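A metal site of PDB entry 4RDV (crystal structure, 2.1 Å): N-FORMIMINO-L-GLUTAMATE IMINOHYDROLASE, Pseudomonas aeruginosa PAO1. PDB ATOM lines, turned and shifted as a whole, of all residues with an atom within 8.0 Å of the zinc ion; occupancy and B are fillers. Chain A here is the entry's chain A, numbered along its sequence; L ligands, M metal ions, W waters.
NE2 of His 269 touches the zinc ion, 3.97 Å away. Within 4 Å of the zinc ion: His 56, His 58, His 232, His 269 and Asp 320.
Water W1 lies within hydrogen-bond range of the side-chain carboxylate (OD2) of Asp 320 (2.5 Å), a ring nitrogen (NE2) of His 269 (2.6 Å) and a nitrogen (N2) of the ligand (2.9 Å).
The side-chain hydroxyl (OH) of Tyr 121 lies within hydrogen-bond range of an oxygen (O1) of the ligand (2.7 Å). An oxygen (O2) of the ligand sits at hydrogen-bond distance from a ring nitrogen (NE2) of His 206, at 2.7 Å. A nitrogen (N2) of the ligand is in salt-bridge range of the side-chain carboxylate of Glu 235, at 3.0 Å. N2 of the ligand is in salt-bridge range of OD2 of Asp 320 (3.6 Å). An oxygen (O1) of the ligand is in hydrogen-bond range of the side-chain amide nitrogen of Gln 61 (3.1 Å).
The zinc ion is bound by water W1 (1.9 Å). NE2 of His 58 is bound to the zinc ion, 2.0 Å away. A ring nitrogen (NE2) of His 56 is bound to the zinc ion, 2.0 Å away. NE2 of His 232 is bound to the zinc ion (2.1 Å). Slightly farther from the zinc ion lies the side-chain carboxylate (OD1) of Asp 320 (2.7 Å).
The side-chain carboxylate of Asp 320 lies close to a ring nitrogen (NE2) of His 269 (3.4 Å). NE2 of His 269 sits close to OE1 of Glu 235 (3.4 Å). The backbone NH of His 58 lies within hydrogen-bond range of the backbone carbonyl oxygen of Asp 320, 3.1 Å away. The backbone carbonyl oxygen (O) of His 56 sits at hydrogen-bond distance from the backbone NH (N) of Ser 319 (3.3 Å). ND1 of His 232 is in hydrogen-bond range of O of His 206 (3.0 Å). The backbone carbonyl oxygen (O) of His 56 sits at hydrogen-bond distance from the backbone NH (N) of Asp 320, 2.9 Å away. O of Phe 119 sits at hydrogen-bond distance from ND1 of His 58, at 3.0 Å.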
ATOM      1  N   HIS A  56       4.827 -13.326  18.387  1.00  0.00           N
ATOM      2  CA  HIS A  56       5.093 -11.891  18.391  1.00  0.00           C
ATOM      3  C   HIS A  56       5.902 -11.421  17.168  1.00  0.00           C
ATOM      4  O   HIS A  56       7.050 -11.824  16.988  1.00  0.00           O
ATOM      5  CB  HIS A  56       5.829 -11.489  19.669  1.00  0.00           C
ATOM      6  CG  HIS A  56       5.946 -10.003  19.864  1.00  0.00           C
ATOM      7  ND1 HIS A  56       4.842  -9.199  20.081  1.00  0.00           N
ATOM      8  CD2 HIS A  56       7.024  -9.179  19.871  1.00  0.00           C
ATOM      9  CE1 HIS A  56       5.240  -7.947  20.226  1.00  0.00           C
ATOM     10  NE2 HIS A  56       6.552  -7.903  20.092  1.00  0.00           N
ATOM     11  N   SER A  57       5.305 -10.555  16.352  1.00  0.00           N
ATOM     12  CA  SER A  57       5.952 -10.084  15.136  1.00  0.00           C
ATOM     13  C   SER A  57       5.601  -8.629  14.798  1.00  0.00           C
ATOM     14  O   SER A  57       4.449  -8.238  14.908  1.00  0.00           O
ATOM     15  CB  SER A  57       5.528 -10.985  13.955  1.00  0.00           C
ATOM     16  OG  SER A  57       5.768 -10.343  12.714  1.00  0.00           O
ATOM     17  N   HIS A  58       6.595  -7.825  14.406  1.00  0.00           N
ATOM     18  CA  HIS A  58       6.315  -6.540  13.722  1.00  0.00           C
ATOM     19  C   HIS A  58       6.918  -6.640  12.323  1.00  0.00           C
ATOM     20  O   HIS A  58       8.119  -6.381  12.133  1.00  0.00           O
ATOM     21  CB  HIS A  58       6.928  -5.341  14.463  1.00  0.00           C
ATOM     22  CG  HIS A  58       6.702  -5.351  15.940  1.00  0.00           C
ATOM     23  ND1 HIS A  58       5.449  -5.309  16.505  1.00  0.00           N
ATOM     24  CD2 HIS A  58       7.578  -5.394  16.966  1.00  0.00           C
ATOM     25  CE1 HIS A  58       5.558  -5.321  17.830  1.00  0.00           C
ATOM     26  NE2 HIS A  58       6.841  -5.367  18.126  1.00  0.00           N
ATOM     27  N   GLN A  61       9.736  -4.569  10.298  1.00  0.00           N
ATOM     28  CA  GLN A  61      11.074  -4.476  10.869  1.00  0.00           C
ATOM     29  C   GLN A  61      12.102  -5.417  10.213  1.00  0.00           C
ATOM     30  O   GLN A  61      13.312  -5.176  10.302  1.00  0.00           O
ATOM     31  CB  GLN A  61      11.022  -4.662  12.393  1.00  0.00           C
ATOM     32  CG  GLN A  61      10.213  -3.547  13.074  1.00  0.00           C
ATOM     33  CD  GLN A  61      10.279  -3.601  14.600  1.00  0.00           C
ATOM     34  OE1 GLN A  61      11.035  -4.374  15.182  1.00  0.00           O
ATOM     35  NE2 GLN A  61       9.468  -2.764  15.241  1.00  0.00           N
ATOM     36  N   PHE A  78      18.498   0.306  23.058  1.00  0.00           N
ATOM     37  CA  PHE A  78      17.112   0.160  22.632  1.00  0.00           C
ATOM     38  C   PHE A  78      16.523   1.484  22.167  1.00  0.00           C
ATOM     39  O   PHE A  78      15.806   1.544  21.177  1.00  0.00           O
ATOM     40  CB  PHE A  78      16.334  -0.384  23.837  1.00  0.00           C
ATOM     41  CG  PHE A  78      14.843  -0.455  23.642  1.00  0.00           C
ATOM     42  CD1 PHE A  78      14.233  -1.672  23.385  1.00  0.00           C
ATOM     43  CD2 PHE A  78      14.050   0.676  23.778  1.00  0.00           C
ATOM     44  CE1 PHE A  78      12.853  -1.749  23.229  1.00  0.00           C
ATOM     45  CE2 PHE A  78      12.672   0.616  23.622  1.00  0.00           C
ATOM     46  CZ  PHE A  78      12.076  -0.603  23.345  1.00  0.00           C
ATOM     47  N   TRP A  81      18.066   2.781  18.952  1.00  0.00           N
ATOM     48  CA  TRP A  81      17.557   1.878  17.927  1.00  0.00           C
ATOM     49  C   TRP A  81      16.136   2.270  17.521  1.00  0.00           C
ATOM     50  O   TRP A  81      15.822   2.292  16.327  1.00  0.00           O
ATOM     51  CB  TRP A  81      17.564   0.431  18.432  1.00  0.00           C
ATOM     52  CG  TRP A  81      16.779  -0.512  17.530  1.00  0.00           C
ATOM     53  CD1 TRP A  81      17.248  -1.195  16.451  1.00  0.00           C
ATOM     54  CD2 TRP A  81      15.393  -0.867  17.661  1.00  0.00           C
ATOM     55  NE1 TRP A  81      16.252  -1.958  15.898  1.00  0.00           N
ATOM     56  CE2 TRP A  81      15.093  -1.764  16.612  1.00  0.00           C
ATOM     57  CE3 TRP A  81      14.370  -0.513  18.550  1.00  0.00           C
ATOM     58  CZ2 TRP A  81      13.824  -2.323  16.436  1.00  0.00           C
ATOM     59  CZ3 TRP A  81      13.103  -1.055  18.374  1.00  0.00           C
ATOM     60  CH2 TRP A  81      12.845  -1.950  17.329  1.00  0.00           C
ATOM     61  N   PHE A 119       1.674  -8.246  15.645  1.00  0.00           N
ATOM     62  CA  PHE A 119       1.438  -7.204  16.635  1.00  0.00           C
ATOM     63  C   PHE A 119       1.538  -5.914  15.822  1.00  0.00           C
ATOM     64  O   PHE A 119       2.614  -5.357  15.632  1.00  0.00           O
ATOM     65  CB  PHE A 119       2.548  -7.313  17.691  1.00  0.00           C
ATOM     66  CG  PHE A 119       2.322  -6.516  18.947  1.00  0.00           C
ATOM     67  CD1 PHE A 119       2.464  -5.132  18.947  1.00  0.00           C
ATOM     68  CD2 PHE A 119       2.074  -7.158  20.152  1.00  0.00           C
ATOM     69  CE1 PHE A 119       2.324  -4.397  20.134  1.00  0.00           C
ATOM     70  CE2 PHE A 119       1.955  -6.431  21.334  1.00  0.00           C
ATOM     71  CZ  PHE A 119       2.068  -5.049  21.324  1.00  0.00           C
ATOM     72  N   TYR A 121       0.921  -2.200  14.585  1.00  0.00           N
ATOM     73  CA  TYR A 121       0.618  -0.815  15.012  1.00  0.00           C
ATOM     74  C   TYR A 121       0.803   0.269  13.939  1.00  0.00           C
ATOM     75  O   TYR A 121       0.631   1.437  14.224  1.00  0.00           O
ATOM     76  CB  TYR A 121       1.421  -0.431  16.269  1.00  0.00           C
ATOM     77  CG  TYR A 121       2.914  -0.651  16.147  1.00  0.00           C
ATOM     78  CD1 TYR A 121       3.696   0.154  15.331  1.00  0.00           C
ATOM     79  CD2 TYR A 121       3.545  -1.671  16.854  1.00  0.00           C
ATOM     80  CE1 TYR A 121       5.070  -0.047  15.219  1.00  0.00           C
ATOM     81  CE2 TYR A 121       4.917  -1.889  16.756  1.00  0.00           C
ATOM     82  CZ  TYR A 121       5.676  -1.065  15.938  1.00  0.00           C
ATOM     83  OH  TYR A 121       7.025  -1.263  15.838  1.00  0.00           O
ATOM     84  N   HIS A 206      -0.274  -1.452  23.003  1.00  0.00           N
ATOM     85  CA  HIS A 206       1.142  -1.465  22.666  1.00  0.00           C
ATOM     86  C   HIS A 206       2.013  -1.687  23.892  1.00  0.00           C
ATOM     87  O   HIS A 206       2.905  -2.527  23.884  1.00  0.00           O
ATOM     88  CB  HIS A 206       1.570  -0.170  21.969  1.00  0.00           C
ATOM     89  CG  HIS A 206       3.051  -0.098  21.736  1.00  0.00           C
ATOM     90  ND1 HIS A 206       3.917   0.413  22.678  1.00  0.00           N
ATOM     91  CD2 HIS A 206       3.828  -0.518  20.704  1.00  0.00           C
ATOM     92  CE1 HIS A 206       5.163   0.330  22.226  1.00  0.00           C
ATOM     93  NE2 HIS A 206       5.125  -0.229  21.020  1.00  0.00           N
ATOM     94  N   ILE A 231       0.273  -7.371  25.079  1.00  0.00           N
ATOM     95  CA  ILE A 231       0.870  -6.094  25.463  1.00  0.00           C
ATOM     96  C   ILE A 231       2.402  -6.253  25.614  1.00  0.00           C
ATOM     97  O   ILE A 231       2.859  -7.267  26.128  1.00  0.00           O
ATOM     98  CB  ILE A 231       0.242  -5.562  26.791  1.00  0.00           C
ATOM     99  CG1 ILE A 231       0.737  -4.163  27.129  1.00  0.00           C
ATOM    100  CG2 ILE A 231       0.511  -6.514  27.969  1.00  0.00           C
ATOM    101  CD1 ILE A 231      -0.044  -3.522  28.286  1.00  0.00           C
ATOM    102  N   HIS A 232       3.191  -5.282  25.130  1.00  0.00           N
ATOM    103  CA  HIS A 232       4.615  -5.238  25.475  1.00  0.00           C
ATOM    104  C   HIS A 232       4.682  -4.816  26.926  1.00  0.00           C
ATOM    105  O   HIS A 232       4.052  -3.836  27.298  1.00  0.00           O
ATOM    106  CB  HIS A 232       5.351  -4.133  24.709  1.00  0.00           C
ATOM    107  CG  HIS A 232       5.577  -4.407  23.262  1.00  0.00           C
ATOM    108  ND1 HIS A 232       5.192  -3.517  22.273  1.00  0.00           N
ATOM    109  CD2 HIS A 232       6.220  -5.417  22.622  1.00  0.00           C
ATOM    110  CE1 HIS A 232       5.566  -3.987  21.091  1.00  0.00           C
ATOM    111  NE2 HIS A 232       6.186  -5.140  21.281  1.00  0.00           N
ATOM    112  N   GLU A 235      10.043  -4.641  29.104  1.00  0.00           N
ATOM    113  CA  GLU A 235      11.180  -4.984  28.240  1.00  0.00           C
ATOM    114  C   GLU A 235      12.493  -4.273  28.646  1.00  0.00           C
ATOM    115  O   GLU A 235      13.566  -4.876  28.652  1.00  0.00           O
ATOM    116  CB  GLU A 235      10.846  -4.698  26.772  1.00  0.00           C
ATOM    117  CG  GLU A 235      11.924  -5.180  25.797  1.00  0.00           C
ATOM    118  CD  GLU A 235      11.650  -4.825  24.341  1.00  0.00           C
ATOM    119  OE1 GLU A 235      10.657  -4.102  24.057  1.00  0.00           O
ATOM    120  OE2 GLU A 235      12.416  -5.285  23.465  1.00  0.00           O
ATOM    121  N   VAL A 268       4.310  -9.660  26.456  1.00  0.00           N
ATOM    122  CA  VAL A 268       5.478  -9.757  25.585  1.00  0.00           C
ATOM    123  C   VAL A 268       6.736  -9.225  26.286  1.00  0.00           C
ATOM    124  O   VAL A 268       6.695  -8.170  26.918  1.00  0.00           O
ATOM    125  CB  VAL A 268       5.222  -9.049  24.241  1.00  0.00           C
ATOM    126  CG1 VAL A 268       6.442  -9.169  23.318  1.00  0.00           C
ATOM    127  CG2 VAL A 268       3.979  -9.635  23.584  1.00  0.00           C
ATOM    128  N   HIS A 269       7.834  -9.965  26.161  1.00  0.00           N
ATOM    129  CA  HIS A 269       9.089  -9.723  26.871  1.00  0.00           C
ATOM    130  C   HIS A 269       9.016 -10.012  28.373  1.00  0.00           C
ATOM    131  O   HIS A 269       9.609 -10.982  28.849  1.00  0.00           O
ATOM    132  CB  HIS A 269       9.686  -8.324  26.600  1.00  0.00           C
ATOM    133  CG  HIS A 269       9.722  -7.968  25.137  1.00  0.00           C
ATOM    134  ND1 HIS A 269      10.384  -8.718  24.205  1.00  0.00           N
ATOM    135  CD2 HIS A 269       9.128  -6.945  24.462  1.00  0.00           C
ATOM    136  CE1 HIS A 269      10.216  -8.183  23.005  1.00  0.00           C
ATOM    137  NE2 HIS A 269       9.454  -7.108  23.137  1.00  0.00           N
ATOM    138  N   CYS A 291      11.152 -13.197  23.205  1.00  0.00           N
ATOM    139  CA  CYS A 291      11.732 -12.981  21.886  1.00  0.00           C
ATOM    140  C   CYS A 291      13.246 -12.883  22.089  1.00  0.00           C
ATOM    141  O   CYS A 291      13.805 -11.800  22.216  1.00  0.00           O
ATOM    142  CB  CYS A 291      11.151 -11.710  21.280  1.00  0.00           C
ATOM    143  SG  CYS A 291       9.322 -11.663  21.358  1.00  0.00           S
ATOM    144  N   THR A 294      15.778 -10.961  19.599  1.00  0.00           N
ATOM    145  CA  THR A 294      15.560  -9.515  19.586  1.00  0.00           C
ATOM    146  C   THR A 294      15.971  -8.898  20.925  1.00  0.00           C
ATOM    147  O   THR A 294      16.609  -7.840  20.974  1.00  0.00           O
ATOM    148  CB  THR A 294      14.094  -9.153  19.227  1.00  0.00           C
ATOM    149  OG1 THR A 294      13.854  -9.446  17.844  1.00  0.00           O
ATOM    150  CG2 THR A 294      13.816  -7.654  19.477  1.00  0.00           C
ATOM    151  N   LEU A 298      18.696  -6.079  21.200  1.00  0.00           N
ATOM    152  CA  LEU A 298      18.343  -4.752  21.736  1.00  0.00           C
ATOM    153  C   LEU A 298      18.927  -4.479  23.123  1.00  0.00           C
ATOM    154  O   LEU A 298      18.692  -3.408  23.701  1.00  0.00           O
ATOM    155  CB  LEU A 298      16.821  -4.576  21.771  1.00  0.00           C
ATOM    156  CG  LEU A 298      16.165  -4.598  20.389  1.00  0.00           C
ATOM    157  CD1 LEU A 298      14.639  -4.433  20.488  1.00  0.00           C
ATOM    158  CD2 LEU A 298      16.766  -3.490  19.518  1.00  0.00           C
ATOM    159  N   SER A 319       9.686 -13.821  17.010  1.00  0.00           N
ATOM    160  CA  SER A 319      10.871 -13.287  16.334  1.00  0.00           C
ATOM    161  C   SER A 319      10.928 -11.755  16.352  1.00  0.00           C
ATOM    162  O   SER A 319      11.971 -11.170  16.067  1.00  0.00           O
ATOM    163  CB  SER A 319      10.958 -13.837  14.905  1.00  0.00           C
ATOM    164  OG  SER A 319       9.834 -13.454  14.144  1.00  0.00           O
ATOM    165  N   ASP A 320       9.800 -11.128  16.696  1.00  0.00           N
ATOM    166  CA  ASP A 320       9.740  -9.704  17.046  1.00  0.00           C
ATOM    167  C   ASP A 320      10.286  -8.741  15.986  1.00  0.00           C
ATOM    168  O   ASP A 320       9.580  -8.391  15.037  1.00  0.00           O
ATOM    169  CB  ASP A 320      10.427  -9.454  18.407  1.00  0.00           C
ATOM    170  CG  ASP A 320      10.145  -8.076  18.964  1.00  0.00           C
ATOM    171  OD1 ASP A 320       9.342  -7.327  18.356  1.00  0.00           O
ATOM    172  OD2 ASP A 320      10.697  -7.724  20.027  1.00  0.00           O
ATOM    173  N   SER A 321      11.532  -8.283  16.154  1.00  0.00           N
ATOM    174  CA  SER A 321      12.166  -7.411  15.153  1.00  0.00           C
ATOM    175  C   SER A 321      12.705  -8.195  13.947  1.00  0.00           C
ATOM    176  O   SER A 321      13.158  -7.599  12.975  1.00  0.00           O
ATOM    177  CB  SER A 321      13.291  -6.569  15.782  1.00  0.00           C
ATOM    178  OG  SER A 321      14.443  -7.355  16.039  1.00  0.00           O
HETATM  179  C1  LIG L   1       7.993  -1.566  19.105  1.00  0.00           C
HETATM  180  N1  LIG L   1       9.892  -2.700  19.938  1.00  0.00           N
HETATM  181  O1  LIG L   1       8.346  -2.080  18.007  1.00  0.00           O
HETATM  182  O2  LIG L   1       6.970  -0.840  19.159  1.00  0.00           O
HETATM  183  C2  LIG L   1       8.814  -1.847  20.320  1.00  0.00           C
HETATM  184  C3  LIG L   1       9.324  -0.543  20.866  1.00  0.00           C
HETATM  185  C4  LIG L   1      10.550  -3.312  21.049  1.00  0.00           C
HETATM  186  N2  LIG L   1      11.450  -4.234  20.773  1.00  0.00           N
HETATM  187  C5  LIG L   1       8.538   0.059  21.987  1.00  0.00           C
HETATM  188  O3  LIG L   1       8.311   1.303  22.018  1.00  0.00           O
HETATM  189  O4  LIG L   1       8.087  -0.694  22.897  1.00  0.00           O
HETATM  190 ZN    ZN M   1       7.421  -6.115  19.878  1.00  0.00          ZN
HETATM  191  O   HOH W   1       9.086  -5.953  20.869  1.00  0.00           O
